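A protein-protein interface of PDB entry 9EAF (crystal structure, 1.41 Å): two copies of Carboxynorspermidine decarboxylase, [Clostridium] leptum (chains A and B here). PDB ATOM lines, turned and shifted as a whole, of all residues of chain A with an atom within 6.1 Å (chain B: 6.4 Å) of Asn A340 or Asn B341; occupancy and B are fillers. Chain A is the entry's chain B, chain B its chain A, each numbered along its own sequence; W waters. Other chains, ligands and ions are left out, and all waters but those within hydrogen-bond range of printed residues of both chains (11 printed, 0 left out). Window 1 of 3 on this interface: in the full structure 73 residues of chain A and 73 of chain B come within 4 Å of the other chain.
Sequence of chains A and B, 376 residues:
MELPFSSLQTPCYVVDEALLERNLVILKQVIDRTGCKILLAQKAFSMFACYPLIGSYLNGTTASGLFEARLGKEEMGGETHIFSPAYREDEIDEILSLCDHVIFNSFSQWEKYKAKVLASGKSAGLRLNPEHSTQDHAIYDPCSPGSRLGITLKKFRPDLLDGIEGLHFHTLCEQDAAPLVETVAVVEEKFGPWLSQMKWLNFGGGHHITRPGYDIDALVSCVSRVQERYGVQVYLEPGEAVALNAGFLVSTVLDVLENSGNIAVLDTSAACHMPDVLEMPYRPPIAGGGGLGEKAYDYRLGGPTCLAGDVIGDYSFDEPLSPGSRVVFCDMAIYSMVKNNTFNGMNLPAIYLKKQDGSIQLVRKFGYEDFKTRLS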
ATOM      1  N   TYR A  13      12.290  13.092   5.899  1.00  0.00           N
ATOM      2  CA  TYR A  13      12.259  14.031   7.012  1.00  0.00           C
ATOM      3  C   TYR A  13      10.906  14.729   7.037  1.00  0.00           C
ATOM      4  O   TYR A  13      10.334  15.039   5.987  1.00  0.00           O
ATOM      5  CB  TYR A  13      13.354  15.096   6.864  1.00  0.00           C
ATOM      6  CG  TYR A  13      14.758  14.555   6.723  1.00  0.00           C
ATOM      7  CD1 TYR A  13      15.486  14.135   7.834  1.00  0.00           C
ATOM      8  CD2 TYR A  13      15.361  14.475   5.479  1.00  0.00           C
ATOM      9  CE1 TYR A  13      16.773  13.636   7.698  1.00  0.00           C
ATOM     10  CE2 TYR A  13      16.631  13.974   5.336  1.00  0.00           C
ATOM     11  CZ  TYR A  13      17.341  13.563   6.439  1.00  0.00           C
ATOM     12  OH  TYR A  13      18.624  13.074   6.255  1.00  0.00           O
ATOM     13  N   CYS A 272      24.223   7.794   5.638  1.00  0.00           N
ATOM     14  CA  CYS A 272      23.797   8.733   4.607  1.00  0.00           C
ATOM     15  C   CYS A 272      22.846   9.801   5.129  1.00  0.00           C
ATOM     16  O   CYS A 272      22.898  10.947   4.673  1.00  0.00           O
ATOM     17  CB  CYS A 272      23.091   7.987   3.469  1.00  0.00           C
ATOM     18  SG  CYS A 272      24.082   6.698   2.698  1.00  0.00           S
ATOM     19  N   HIS A 273      21.962   9.448   6.063  1.00  0.00           N
ATOM     20  CA  HIS A 273      20.815  10.286   6.385  1.00  0.00           C
ATOM     21  C   HIS A 273      20.853  10.895   7.774  1.00  0.00           C
ATOM     22  O   HIS A 273      20.132  11.869   8.023  1.00  0.00           O
ATOM     23  CB  HIS A 273      19.525   9.470   6.234  1.00  0.00           C
ATOM     24  CG  HIS A 273      19.347   8.894   4.869  1.00  0.00           C
ATOM     25  ND1 HIS A 273      18.527   7.816   4.610  1.00  0.00           N
ATOM     26  CD2 HIS A 273      19.889   9.250   3.682  1.00  0.00           C
ATOM     27  CE1 HIS A 273      18.569   7.539   3.318  1.00  0.00           C
ATOM     28  NE2 HIS A 273      19.390   8.394   2.734  1.00  0.00           N
ATOM     29  N   MET A 274      21.647  10.349   8.688  1.00  0.00           N
ATOM     30  CA  MET A 274      21.840  10.948  10.011  1.00  0.00           C
ATOM     31  C   MET A 274      23.267  10.662  10.438  1.00  0.00           C
ATOM     32  O   MET A 274      23.519   9.951  11.418  1.00  0.00           O
ATOM     33  CB  MET A 274      20.820  10.428  11.023  1.00  0.00           C
ATOM     34  CG  MET A 274      20.368   9.018  10.816  1.00  0.00           C
ATOM     35  SD  MET A 274      18.978   8.544  11.870  1.00  0.00           S
ATOM     36  CE  MET A 274      18.709   6.917  11.200  1.00  0.00           C
ATOM     37  N   PRO A 275      24.236  11.220   9.716  1.00  0.00           N
ATOM     38  CA  PRO A 275      25.630  10.794   9.900  1.00  0.00           C
ATOM     39  C   PRO A 275      26.170  11.021  11.300  1.00  0.00           C
ATOM     40  O   PRO A 275      27.067  10.285  11.725  1.00  0.00           O
ATOM     41  CB  PRO A 275      26.388  11.600   8.836  1.00  0.00           C
ATOM     42  CG  PRO A 275      25.487  12.752   8.506  1.00  0.00           C
ATOM     43  CD  PRO A 275      24.092  12.252   8.679  1.00  0.00           C
ATOM     44  N   SER A 336      21.221  17.516  10.199  1.00  0.00           N
ATOM     45  CA  SER A 336      20.824  16.326   9.454  1.00  0.00           C
ATOM     46  C   SER A 336      20.766  16.641   7.963  1.00  0.00           C
ATOM     47  O   SER A 336      21.697  16.320   7.218  1.00  0.00           O
ATOM     48  CB  SER A 336      19.459  15.827   9.940  1.00  0.00           C
ATOM     49  OG  SER A 336      18.501  16.873   9.915  1.00  0.00           O
ATOM     50  N   MET A 337      19.679  17.282   7.524  1.00  0.00           N
ATOM     51  CA  MET A 337      19.524  17.627   6.114  1.00  0.00           C
ATOM     52  C   MET A 337      20.653  18.520   5.617  1.00  0.00           C
ATOM     53  O   MET A 337      20.999  18.480   4.428  1.00  0.00           O
ATOM     54  CB  MET A 337      18.181  18.330   5.904  1.00  0.00           C
ATOM     55  CG  MET A 337      16.974  17.405   5.941  1.00  0.00           C
ATOM     56  SD  MET A 337      15.398  18.284   6.071  1.00  0.00           S
ATOM     57  CE  MET A 337      15.415  18.730   7.808  1.00  0.00           C
ATOM     58  N   VAL A 338      21.236  19.335   6.502  1.00  0.00           N
ATOM     59  CA  VAL A 338      22.314  20.241   6.115  1.00  0.00           C
ATOM     60  C   VAL A 338      23.613  19.524   5.795  1.00  0.00           C
ATOM     61  O   VAL A 338      24.540  20.154   5.265  1.00  0.00           O
ATOM     62  CB  VAL A 338      22.635  21.270   7.221  1.00  0.00           C
ATOM     63  CG1 VAL A 338      21.506  22.274   7.362  1.00  0.00           C
ATOM     64  CG2 VAL A 338      22.933  20.562   8.549  1.00  0.00           C
ATOM     65  N   LYS A 339      23.725  18.233   6.117  1.00  0.00           N
ATOM     66  CA  LYS A 339      25.002  17.551   5.935  1.00  0.00           C
ATOM     67  C   LYS A 339      24.852  16.117   5.438  1.00  0.00           C
ATOM     68  O   LYS A 339      25.806  15.336   5.550  1.00  0.00           O
ATOM     69  CB  LYS A 339      25.815  17.565   7.238  1.00  0.00           C
ATOM     70  CG  LYS A 339      25.158  16.818   8.390  1.00  0.00           C
ATOM     71  CD  LYS A 339      25.874  17.051   9.718  1.00  0.00           C
ATOM     72  CE  LYS A 339      27.330  16.625   9.689  1.00  0.00           C
ATOM     73  NZ  LYS A 339      27.952  16.793  11.028  1.00  0.00           N
ATOM     74  N   ASN A 340      23.702  15.744   4.879  1.00  0.00           N
ATOM     75  CA  ASN A 340      23.520  14.366   4.441  1.00  0.00           C
ATOM     76  C   ASN A 340      24.177  14.141   3.077  1.00  0.00           C
ATOM     77  O   ASN A 340      24.733  15.056   2.466  1.00  0.00           O
ATOM     78  CB  ASN A 340      22.051  13.943   4.553  1.00  0.00           C
ATOM     79  CG  ASN A 340      21.104  14.733   3.661  1.00  0.00           C
ATOM     80  OD1 ASN A 340      21.514  15.487   2.787  1.00  0.00           O
ATOM     81  ND2 ASN A 340      19.805  14.529   3.876  1.00  0.00           N
ATOM     82  N   ASN A 341      24.165  12.893   2.608  1.00  0.00           N
ATOM     83  CA  ASN A 341      24.989  12.515   1.470  1.00  0.00           C
ATOM     84  C   ASN A 341      24.348  11.349   0.728  1.00  0.00           C
ATOM     85  O   ASN A 341      23.365  10.761   1.180  1.00  0.00           O
ATOM     86  CB  ASN A 341      26.398  12.145   1.939  1.00  0.00           C
ATOM     87  CG  ASN A 341      26.403  10.910   2.807  1.00  0.00           C
ATOM     88  OD1 ASN A 341      26.183   9.801   2.318  1.00  0.00           O
ATOM     89  ND2 ASN A 341      26.649  11.088   4.098  1.00  0.00           N
ATOM     90  N   THR A 342      24.930  11.018  -0.430  1.00  0.00           N
ATOM     91  CA  THR A 342      24.455   9.943  -1.298  1.00  0.00           C
ATOM     92  C   THR A 342      25.470   8.804  -1.399  1.00  0.00           C
ATOM     93  O   THR A 342      25.575   8.145  -2.437  1.00  0.00           O
ATOM     94  CB  THR A 342      24.109  10.475  -2.691  1.00  0.00           C
ATOM     95  OG1 THR A 342      25.185  11.287  -3.180  1.00  0.00           O
ATOM     96  CG2 THR A 342      22.837  11.296  -2.652  1.00  0.00           C
ATOM     97  N   LEU A 348      18.396  10.329  -1.380  1.00  0.00           N
ATOM     98  CA  LEU A 348      18.176  11.212  -0.248  1.00  0.00           C
ATOM     99  C   LEU A 348      16.729  11.100   0.227  1.00  0.00           C
ATOM    100  O   LEU A 348      15.815  10.906  -0.577  1.00  0.00           O
ATOM    101  CB  LEU A 348      18.446  12.648  -0.669  1.00  0.00           C
ATOM    102  CG  LEU A 348      19.913  12.905  -1.009  1.00  0.00           C
ATOM    103  CD1 LEU A 348      20.045  14.055  -1.990  1.00  0.00           C
ATOM    104  CD2 LEU A 348      20.711  13.174   0.255  1.00  0.00           C
ATOM    105  N   PRO A 349      16.488  11.217   1.528  1.00  0.00           N
ATOM    106  CA  PRO A 349      15.105  11.200   2.008  1.00  0.00           C
ATOM    107  C   PRO A 349      14.349  12.413   1.501  1.00  0.00           C
ATOM    108  O   PRO A 349      14.906  13.504   1.347  1.00  0.00           O
ATOM    109  CB  PRO A 349      15.250  11.246   3.534  1.00  0.00           C
ATOM    110  CG  PRO A 349      16.664  10.843   3.806  1.00  0.00           C
ATOM    111  CD  PRO A 349      17.448  11.347   2.633  1.00  0.00           C
ATOM    112  N   ARG A 374      26.796  14.777  -8.779  1.00  0.00           N
ATOM    113  CA  ARG A 374      27.897  15.033  -7.862  1.00  0.00           C
ATOM    114  C   ARG A 374      29.183  14.317  -8.254  1.00  0.00           C
ATOM    115  O   ARG A 374      30.217  14.553  -7.626  1.00  0.00           O
ATOM    116  CB  ARG A 374      27.492  14.603  -6.444  1.00  0.00           C
ATOM    117  CG  ARG A 374      26.364  15.430  -5.839  1.00  0.00           C
ATOM    118  CD  ARG A 374      26.799  16.889  -5.639  1.00  0.00           C
ATOM    119  NE  ARG A 374      25.773  17.743  -5.045  1.00  0.00           N
ATOM    120  CZ  ARG A 374      25.562  17.871  -3.743  1.00  0.00           C
ATOM    121  NH1 ARG A 374      26.249  17.167  -2.858  1.00  0.00           N
ATOM    122  NH2 ARG A 374      24.641  18.731  -3.318  1.00  0.00           N
ATOM    123  N   ALA B 270      37.886  19.208   5.896  1.00  0.00           N
ATOM    124  CA  ALA B 270      37.815  17.766   6.106  1.00  0.00           C
ATOM    125  C   ALA B 270      36.370  17.321   6.284  1.00  0.00           C
ATOM    126  O   ALA B 270      35.923  16.359   5.648  1.00  0.00           O
ATOM    127  CB  ALA B 270      38.658  17.354   7.310  1.00  0.00           C
ATOM    128  N   ALA B 271      35.615  18.035   7.126  1.00  0.00           N
ATOM    129  CA  ALA B 271      34.228  17.658   7.390  1.00  0.00           C
ATOM    130  C   ALA B 271      33.417  17.556   6.105  1.00  0.00           C
ATOM    131  O   ALA B 271      32.551  16.683   5.977  1.00  0.00           O
ATOM    132  CB  ALA B 271      33.583  18.682   8.326  1.00  0.00           C
ATOM    133  N   CYS B 272      33.660  18.457   5.153  1.00  0.00           N
ATOM    134  CA  CYS B 272      32.858  18.518   3.937  1.00  0.00           C
ATOM    135  C   CYS B 272      33.461  17.734   2.778  1.00  0.00           C
ATOM    136  O   CYS B 272      32.719  17.165   1.973  1.00  0.00           O
ATOM    137  CB  CYS B 272      32.704  19.971   3.485  1.00  0.00           C
ATOM    138  SG  CYS B 272      31.932  21.055   4.688  1.00  0.00           S
ATOM    139  N   HIS B 273      34.789  17.717   2.655  1.00  0.00           N
ATOM    140  CA  HIS B 273      35.440  17.262   1.432  1.00  0.00           C
ATOM    141  C   HIS B 273      36.244  15.983   1.585  1.00  0.00           C
ATOM    142  O   HIS B 273      36.547  15.335   0.575  1.00  0.00           O
ATOM    143  CB  HIS B 273      36.356  18.370   0.898  1.00  0.00           C
ATOM    144  CG  HIS B 273      35.638  19.657   0.655  1.00  0.00           C
ATOM    145  ND1 HIS B 273      36.274  20.878   0.611  1.00  0.00           N
ATOM    146  CD2 HIS B 273      34.324  19.909   0.450  1.00  0.00           C
ATOM    147  CE1 HIS B 273      35.381  21.826   0.384  1.00  0.00           C
ATOM    148  NE2 HIS B 273      34.191  21.262   0.278  1.00  0.00           N
ATOM    149  N   PRO B 275      35.507  13.523   4.546  1.00  0.00           N
ATOM    150  CA  PRO B 275      34.939  13.296   5.879  1.00  0.00           C
ATOM    151  C   PRO B 275      35.561  12.130   6.624  1.00  0.00           C
ATOM    152  O   PRO B 275      35.595  12.150   7.858  1.00  0.00           O
ATOM    153  CB  PRO B 275      33.444  13.085   5.598  1.00  0.00           C
ATOM    154  CG  PRO B 275      33.367  12.725   4.158  1.00  0.00           C
ATOM    155  CD  PRO B 275      34.501  13.414   3.480  1.00  0.00           C
ATOM    156  N   SER B 336      35.663   9.457  -1.250  1.00  0.00           N
ATOM    157  CA  SER B 336      35.747  10.898  -1.062  1.00  0.00           C
ATOM    158  C   SER B 336      34.596  11.576  -1.790  1.00  0.00           C
ATOM    159  O   SER B 336      33.598  11.946  -1.166  1.00  0.00           O
ATOM    160  CB  SER B 336      37.091  11.415  -1.584  1.00  0.00           C
ATOM    161  OG  SER B 336      37.284  10.998  -2.921  1.00  0.00           O
ATOM    162  N   LYS B 339      30.935  10.584  -1.187  1.00  0.00           N
ATOM    163  CA  LYS B 339      30.266  10.782   0.094  1.00  0.00           C
ATOM    164  C   LYS B 339      30.472  12.183   0.655  1.00  0.00           C
ATOM    165  O   LYS B 339      30.241  12.396   1.852  1.00  0.00           O
ATOM    166  CB  LYS B 339      30.722   9.731   1.126  1.00  0.00           C
ATOM    167  CG  LYS B 339      32.204   9.789   1.483  1.00  0.00           C
ATOM    168  CD  LYS B 339      32.650   8.619   2.363  1.00  0.00           C
ATOM    169  CE  LYS B 339      31.762   8.423   3.585  1.00  0.00           C
ATOM    170  NZ  LYS B 339      32.388   7.477   4.547  1.00  0.00           N
ATOM    171  N   ASN B 340      30.886  13.148  -0.163  1.00  0.00           N
ATOM    172  CA  ASN B 340      31.103  14.488   0.364  1.00  0.00           C
ATOM    173  C   ASN B 340      29.776  15.234   0.506  1.00  0.00           C
ATOM    174  O   ASN B 340      28.705  14.728   0.159  1.00  0.00           O
ATOM    175  CB  ASN B 340      32.178  15.239  -0.434  1.00  0.00           C
ATOM    176  CG  ASN B 340      31.826  15.471  -1.897  1.00  0.00           C
ATOM    177  OD1 ASN B 340      30.695  15.284  -2.333  1.00  0.00           O
ATOM    178  ND2 ASN B 340      32.822  15.923  -2.664  1.00  0.00           N
ATOM    179  N   ASN B 341      29.843  16.437   1.077  1.00  0.00           N
ATOM    180  CA  ASN B 341      28.638  17.126   1.520  1.00  0.00           C
ATOM    181  C   ASN B 341      28.851  18.636   1.479  1.00  0.00           C
ATOM    182  O   ASN B 341      29.959  19.125   1.249  1.00  0.00           O
ATOM    183  CB  ASN B 341      28.246  16.674   2.930  1.00  0.00           C
ATOM    184  CG  ASN B 341      29.273  17.066   3.966  1.00  0.00           C
ATOM    185  OD1 ASN B 341      29.418  18.243   4.285  1.00  0.00           O
ATOM    186  ND2 ASN B 341      30.008  16.089   4.483  1.00  0.00           N
ATOM    187  N   THR B 342      27.760  19.372   1.722  1.00  0.00           N
ATOM    188  CA  THR B 342      27.740  20.833   1.704  1.00  0.00           C
ATOM    189  C   THR B 342      27.423  21.417   3.080  1.00  0.00           C
ATOM    190  O   THR B 342      26.810  22.485   3.181  1.00  0.00           O
ATOM    191  CB  THR B 342      26.749  21.364   0.665  1.00  0.00           C
ATOM    192  OG1 THR B 342      25.485  20.703   0.814  1.00  0.00           O
ATOM    193  CG2 THR B 342      27.259  21.132  -0.747  1.00  0.00           C
ATOM    194  N   PHE B 343      27.836  20.732   4.145  1.00  0.00           N
ATOM    195  CA  PHE B 343      27.676  21.248   5.501  1.00  0.00           C
ATOM    196  C   PHE B 343      28.310  22.634   5.596  1.00  0.00           C
ATOM    197  O   PHE B 343      29.320  22.916   4.948  1.00  0.00           O
ATOM    198  CB  PHE B 343      28.368  20.265   6.452  1.00  0.00           C
ATOM    199  CG  PHE B 343      28.108  20.493   7.921  1.00  0.00           C
ATOM    200  CD1 PHE B 343      26.918  21.029   8.386  1.00  0.00           C
ATOM    201  CD2 PHE B 343      29.075  20.127   8.846  1.00  0.00           C
ATOM    202  CE1 PHE B 343      26.713  21.208   9.752  1.00  0.00           C
ATOM    203  CE2 PHE B 343      28.874  20.300  10.202  1.00  0.00           C
ATOM    204  CZ  PHE B 343      27.696  20.841  10.655  1.00  0.00           C
ATOM    205  N   ASN B 344      27.693  23.522   6.382  1.00  0.00           N
ATOM    206  CA  ASN B 344      28.108  24.920   6.519  1.00  0.00           C
ATOM    207  C   ASN B 344      27.937  25.715   5.232  1.00  0.00           C
ATOM    208  O   ASN B 344      28.375  26.878   5.164  1.00  0.00           O
ATOM    209  CB  ASN B 344      29.569  25.081   6.961  1.00  0.00           C
ATOM    210  CG  ASN B 344      29.792  24.803   8.427  1.00  0.00           C
ATOM    211  OD1 ASN B 344      30.544  25.519   9.090  1.00  0.00           O
ATOM    212  ND2 ASN B 344      29.183  23.748   8.933  1.00  0.00           N
ATOM    213  N   MET B 346      29.544  25.082   2.503  1.00  0.00           N
ATOM    214  CA  MET B 346      30.772  25.091   1.718  1.00  0.00           C
ATOM    215  C   MET B 346      30.497  24.578   0.311  1.00  0.00           C
ATOM    216  O   MET B 346      29.799  23.580   0.117  1.00  0.00           O
ATOM    217  CB  MET B 346      31.849  24.227   2.375  1.00  0.00           C
ATOM    218  CG  MET B 346      32.258  24.653   3.783  1.00  0.00           C
ATOM    219  SD  MET B 346      33.055  26.276   3.877  1.00  0.00           S
ATOM    220  CE  MET B 346      31.616  27.333   4.134  1.00  0.00           C
ATOM    221  N   ASN B 347      31.044  25.273  -0.681  1.00  0.00           N
ATOM    222  CA  ASN B 347      30.926  24.806  -2.054  1.00  0.00           C
ATOM    223  C   ASN B 347      31.711  23.514  -2.226  1.00  0.00           C
ATOM    224  O   ASN B 347      32.781  23.335  -1.640  1.00  0.00           O
ATOM    225  CB  ASN B 347      31.463  25.864  -3.019  1.00  0.00           C
ATOM    226  CG  ASN B 347      31.045  25.609  -4.454  1.00  0.00           C
ATOM    227  OD1 ASN B 347      30.043  24.950  -4.714  1.00  0.00           O
ATOM    228  ND2 ASN B 347      31.810  26.137  -5.390  1.00  0.00           N
ATOM    229  N   LEU B 348      31.169  22.608  -3.031  1.00  0.00           N
ATOM    230  CA  LEU B 348      31.857  21.358  -3.311  1.00  0.00           C
ATOM    231  C   LEU B 348      33.111  21.628  -4.137  1.00  0.00           C
ATOM    232  O   LEU B 348      33.113  22.515  -4.993  1.00  0.00           O
ATOM    233  CB  LEU B 348      30.928  20.447  -4.097  1.00  0.00           C
ATOM    234  CG  LEU B 348      29.715  20.006  -3.284  1.00  0.00           C
ATOM    235  CD1 LEU B 348      28.541  19.681  -4.189  1.00  0.00           C
ATOM    236  CD2 LEU B 348      30.084  18.808  -2.426  1.00  0.00           C
ATOM    237  N   PRO B 349      34.188  20.879  -3.918  1.00  0.00           N
ATOM    238  CA  PRO B 349      35.376  21.060  -4.754  1.00  0.00           C
ATOM    239  C   PRO B 349      35.074  20.695  -6.200  1.00  0.00           C
ATOM    240  O   PRO B 349      34.287  19.788  -6.486  1.00  0.00           O
ATOM    241  CB  PRO B 349      36.398  20.089  -4.142  1.00  0.00           C
ATOM    242  CG  PRO B 349      35.863  19.742  -2.788  1.00  0.00           C
ATOM    243  CD  PRO B 349      34.371  19.816  -2.920  1.00  0.00           C
ATOM    244  N   ARG B 374      19.301  20.942  -1.961  1.00  0.00           N
ATOM    245  CA  ARG B 374      19.224  19.857  -0.994  1.00  0.00           C
ATOM    246  C   ARG B 374      18.392  20.208   0.235  1.00  0.00           C
ATOM    247  O   ARG B 374      18.137  19.326   1.061  1.00  0.00           O
ATOM    248  CB  ARG B 374      20.641  19.473  -0.555  1.00  0.00           C
ATOM    249  CG  ARG B 374      21.491  18.869  -1.670  1.00  0.00           C
ATOM    250  CD  ARG B 374      20.905  17.546  -2.162  1.00  0.00           C
ATOM    251  NE  ARG B 374      21.699  16.897  -3.201  1.00  0.00           N
ATOM    252  CZ  ARG B 374      22.728  16.092  -2.972  1.00  0.00           C
ATOM    253  NH1 ARG B 374      23.166  15.861  -1.745  1.00  0.00           N
ATOM    254  NH2 ARG B 374      23.328  15.498  -4.001  1.00  0.00           N
HETATM  255  O   HOH W   1      22.690  16.959   0.811  1.00  0.00           O
HETATM  256  O   HOH W   2      28.129  15.035  -3.015  1.00  0.00           O
HETATM  257  O   HOH W   3      23.672  22.704   4.098  1.00  0.00           O
HETATM  258  O   HOH W   4      22.742  19.227   2.388  1.00  0.00           O
HETATM  259  O   HOH W   5      19.076  16.652   1.234  1.00  0.00           O
HETATM  260  O   HOH W   6      30.635  16.110  -5.323  1.00  0.00           O
HETATM  261  O   HOH W   7      24.982  18.394  -0.491  1.00  0.00           O
HETATM  262  O   HOH W   8      25.937  15.493  -0.036  1.00  0.00           O
HETATM  263  O   HOH W   9      25.243  17.939   2.629  1.00  0.00           O
HETATM  264  O   HOH W  10      25.303  13.959  -2.616  1.00  0.00           O
HETATM  265  O   HOH W  11      27.577  12.373  -1.096  1.00  0.00           O
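Thr B342 touches Val A338 (C to O, 3.8 Å). O of Val A338 touches CA of Phe B343, at 3.3 Å. Lys A339 touches Asn B341. CE2 of Phe B343 touches NZ of Lys A339 (3.7 Å). CB of Asn B341 touches O of Asn A340, 3.9 Å away. Asn A341 touches Lys B339. CB of Asn A341 touches O of Asn B340, at 3.9 Å. Arg B374 touches Leu A348. NE of Arg A374 touches CD1 of Leu B348, 3.5 Å away.
Hydrophobic or aromatic side chains of chain A that line the printed part of chain B: Leu A348. Along chain A the printed residues that touch a printed residue of chain B span positions 338 to 374. Printed residues of chain B that touch a printed residue of chain A: Lys B339, Asn B340, Asn B341, Thr B342, Phe B343, Leu B348 and Arg B374. Hydrophobic or aromatic side chains of chain B within 4 Å of the printed part of chain A: Phe B343 and Leu B348. Among the printed residues, 10 pairs touch across the chains. Among the printed residues, no Asp or Glu carboxylate lies within 4 Å of a Lys or Arg side-chain nitrogen of the other chain.
The backbone NH (N) of Asn B341 sits at hydrogen-bond distance from the backbone carbonyl oxygen (O) of Cys B272 (3.1 Å). The side-chain sulfur of Cys B272 sits at hydrogen-bond distance from the backbone carbonyl oxygen of Phe B343, at 3.2 Å. The side-chain amide oxygen of Asn B341 sits at hydrogen-bond distance from the backbone NH of Phe B343 (3.0 Å). The side-chain hydroxyl (OH) of Tyr A13 is in hydrogen-bond range of the side-chain amide nitrogen (ND2) of Asn A340. N of Asn A341 sits at hydrogen-bond distance from O of Cys A272. The side-chain amide oxygen of Asn A340 sits close to the backbone carbonyl oxygen of Met A337, 3.5 Å away.
The guanidinium group of Arg A374 lies close to the guanidinium group of Arg B374.
Met A337 touches none of the printed residues of chain B. Of the printed residues of chain B, Val A338 touches Thr B342 (3.8 Å) and Phe B343 (3.3 Å). Of the printed residues of chain B, Lys A339 touches Asn B341 and Phe B343. Asn A340 touches just one residue of chain B: Asn B341. Printed residues of chain A within 4 Å of Lys B339: Asn A341. Of the printed residues of chain A, Asn B340 touches Asn A341. Asn B341 touches just these residues of chain A: Lys A339 (3.8 Å) and Asn A340 (3.9 Å). Printed residues of chain A within 4 Å of Leu B348: Arg A374 (3.5 Å). The nearest residue of chain B that does not touch Asn A340 is Arg B374 (4.6 Å). The nearest printed residue of chain A that does not touch Asn B341 is Arg A374 (5.0 Å). The nearest printed residue of chain B that does not touch Lys A339 is Thr B342 (5.4 Å).
Lys A339 touches Asn B341, and with the chains exchanged Asn A341 touches Lys B339. Asn A340 touches Asn B341, and with the chains exchanged Asn A341 touches Asn B340. Leu A348 touches Arg B374, and with the chains exchanged Arg A374 touches Leu B348. Arg A374 touches its own counterpart, Arg B374. Of the 10 pairs that touch across the chains among the printed residues, 7 have their exchanged pair printed and touching as well.
Water W2 bridges OD1 of Asn B340 and NH1 of Arg A374. Water W7 lies within hydrogen-bond range of the side-chain hydroxyl (OG1) of Thr B342 (2.7 Å), the guanidinium group (NH2) of Arg A374 (2.9 Å) and the guanidinium group (NH1) of Arg B374 (3.4 Å). Water W1 lies within hydrogen-bond range of the side-chain amide oxygen (OD1) of Asn A340 (2.7 Å) and the guanidinium group (NH1) of Arg B374 (2.8 Å). Water W10 lies within hydrogen-bond range of the side-chain hydroxyl (OG1) of Thr A342 (2.7 Å), the guanidinium group (NH2) of Arg B374 (2.9 Å) and the guanidinium group (NH1) of Arg A374 (3.4 Å). Water W4 lies within hydrogen-bond range of the backbone carbonyl oxygen (O) of Met A337 (2.8 Å) and the side-chain hydroxyl (OG1) of Thr B342 (3.5 Å). Water W8 lies within hydrogen-bond range of O of Asn A340 (2.8 Å), O of Asn B340 (2.9 Å), NH1 of Arg B374 (3.3 Å) and NH1 of Arg A374 (3.3 Å).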
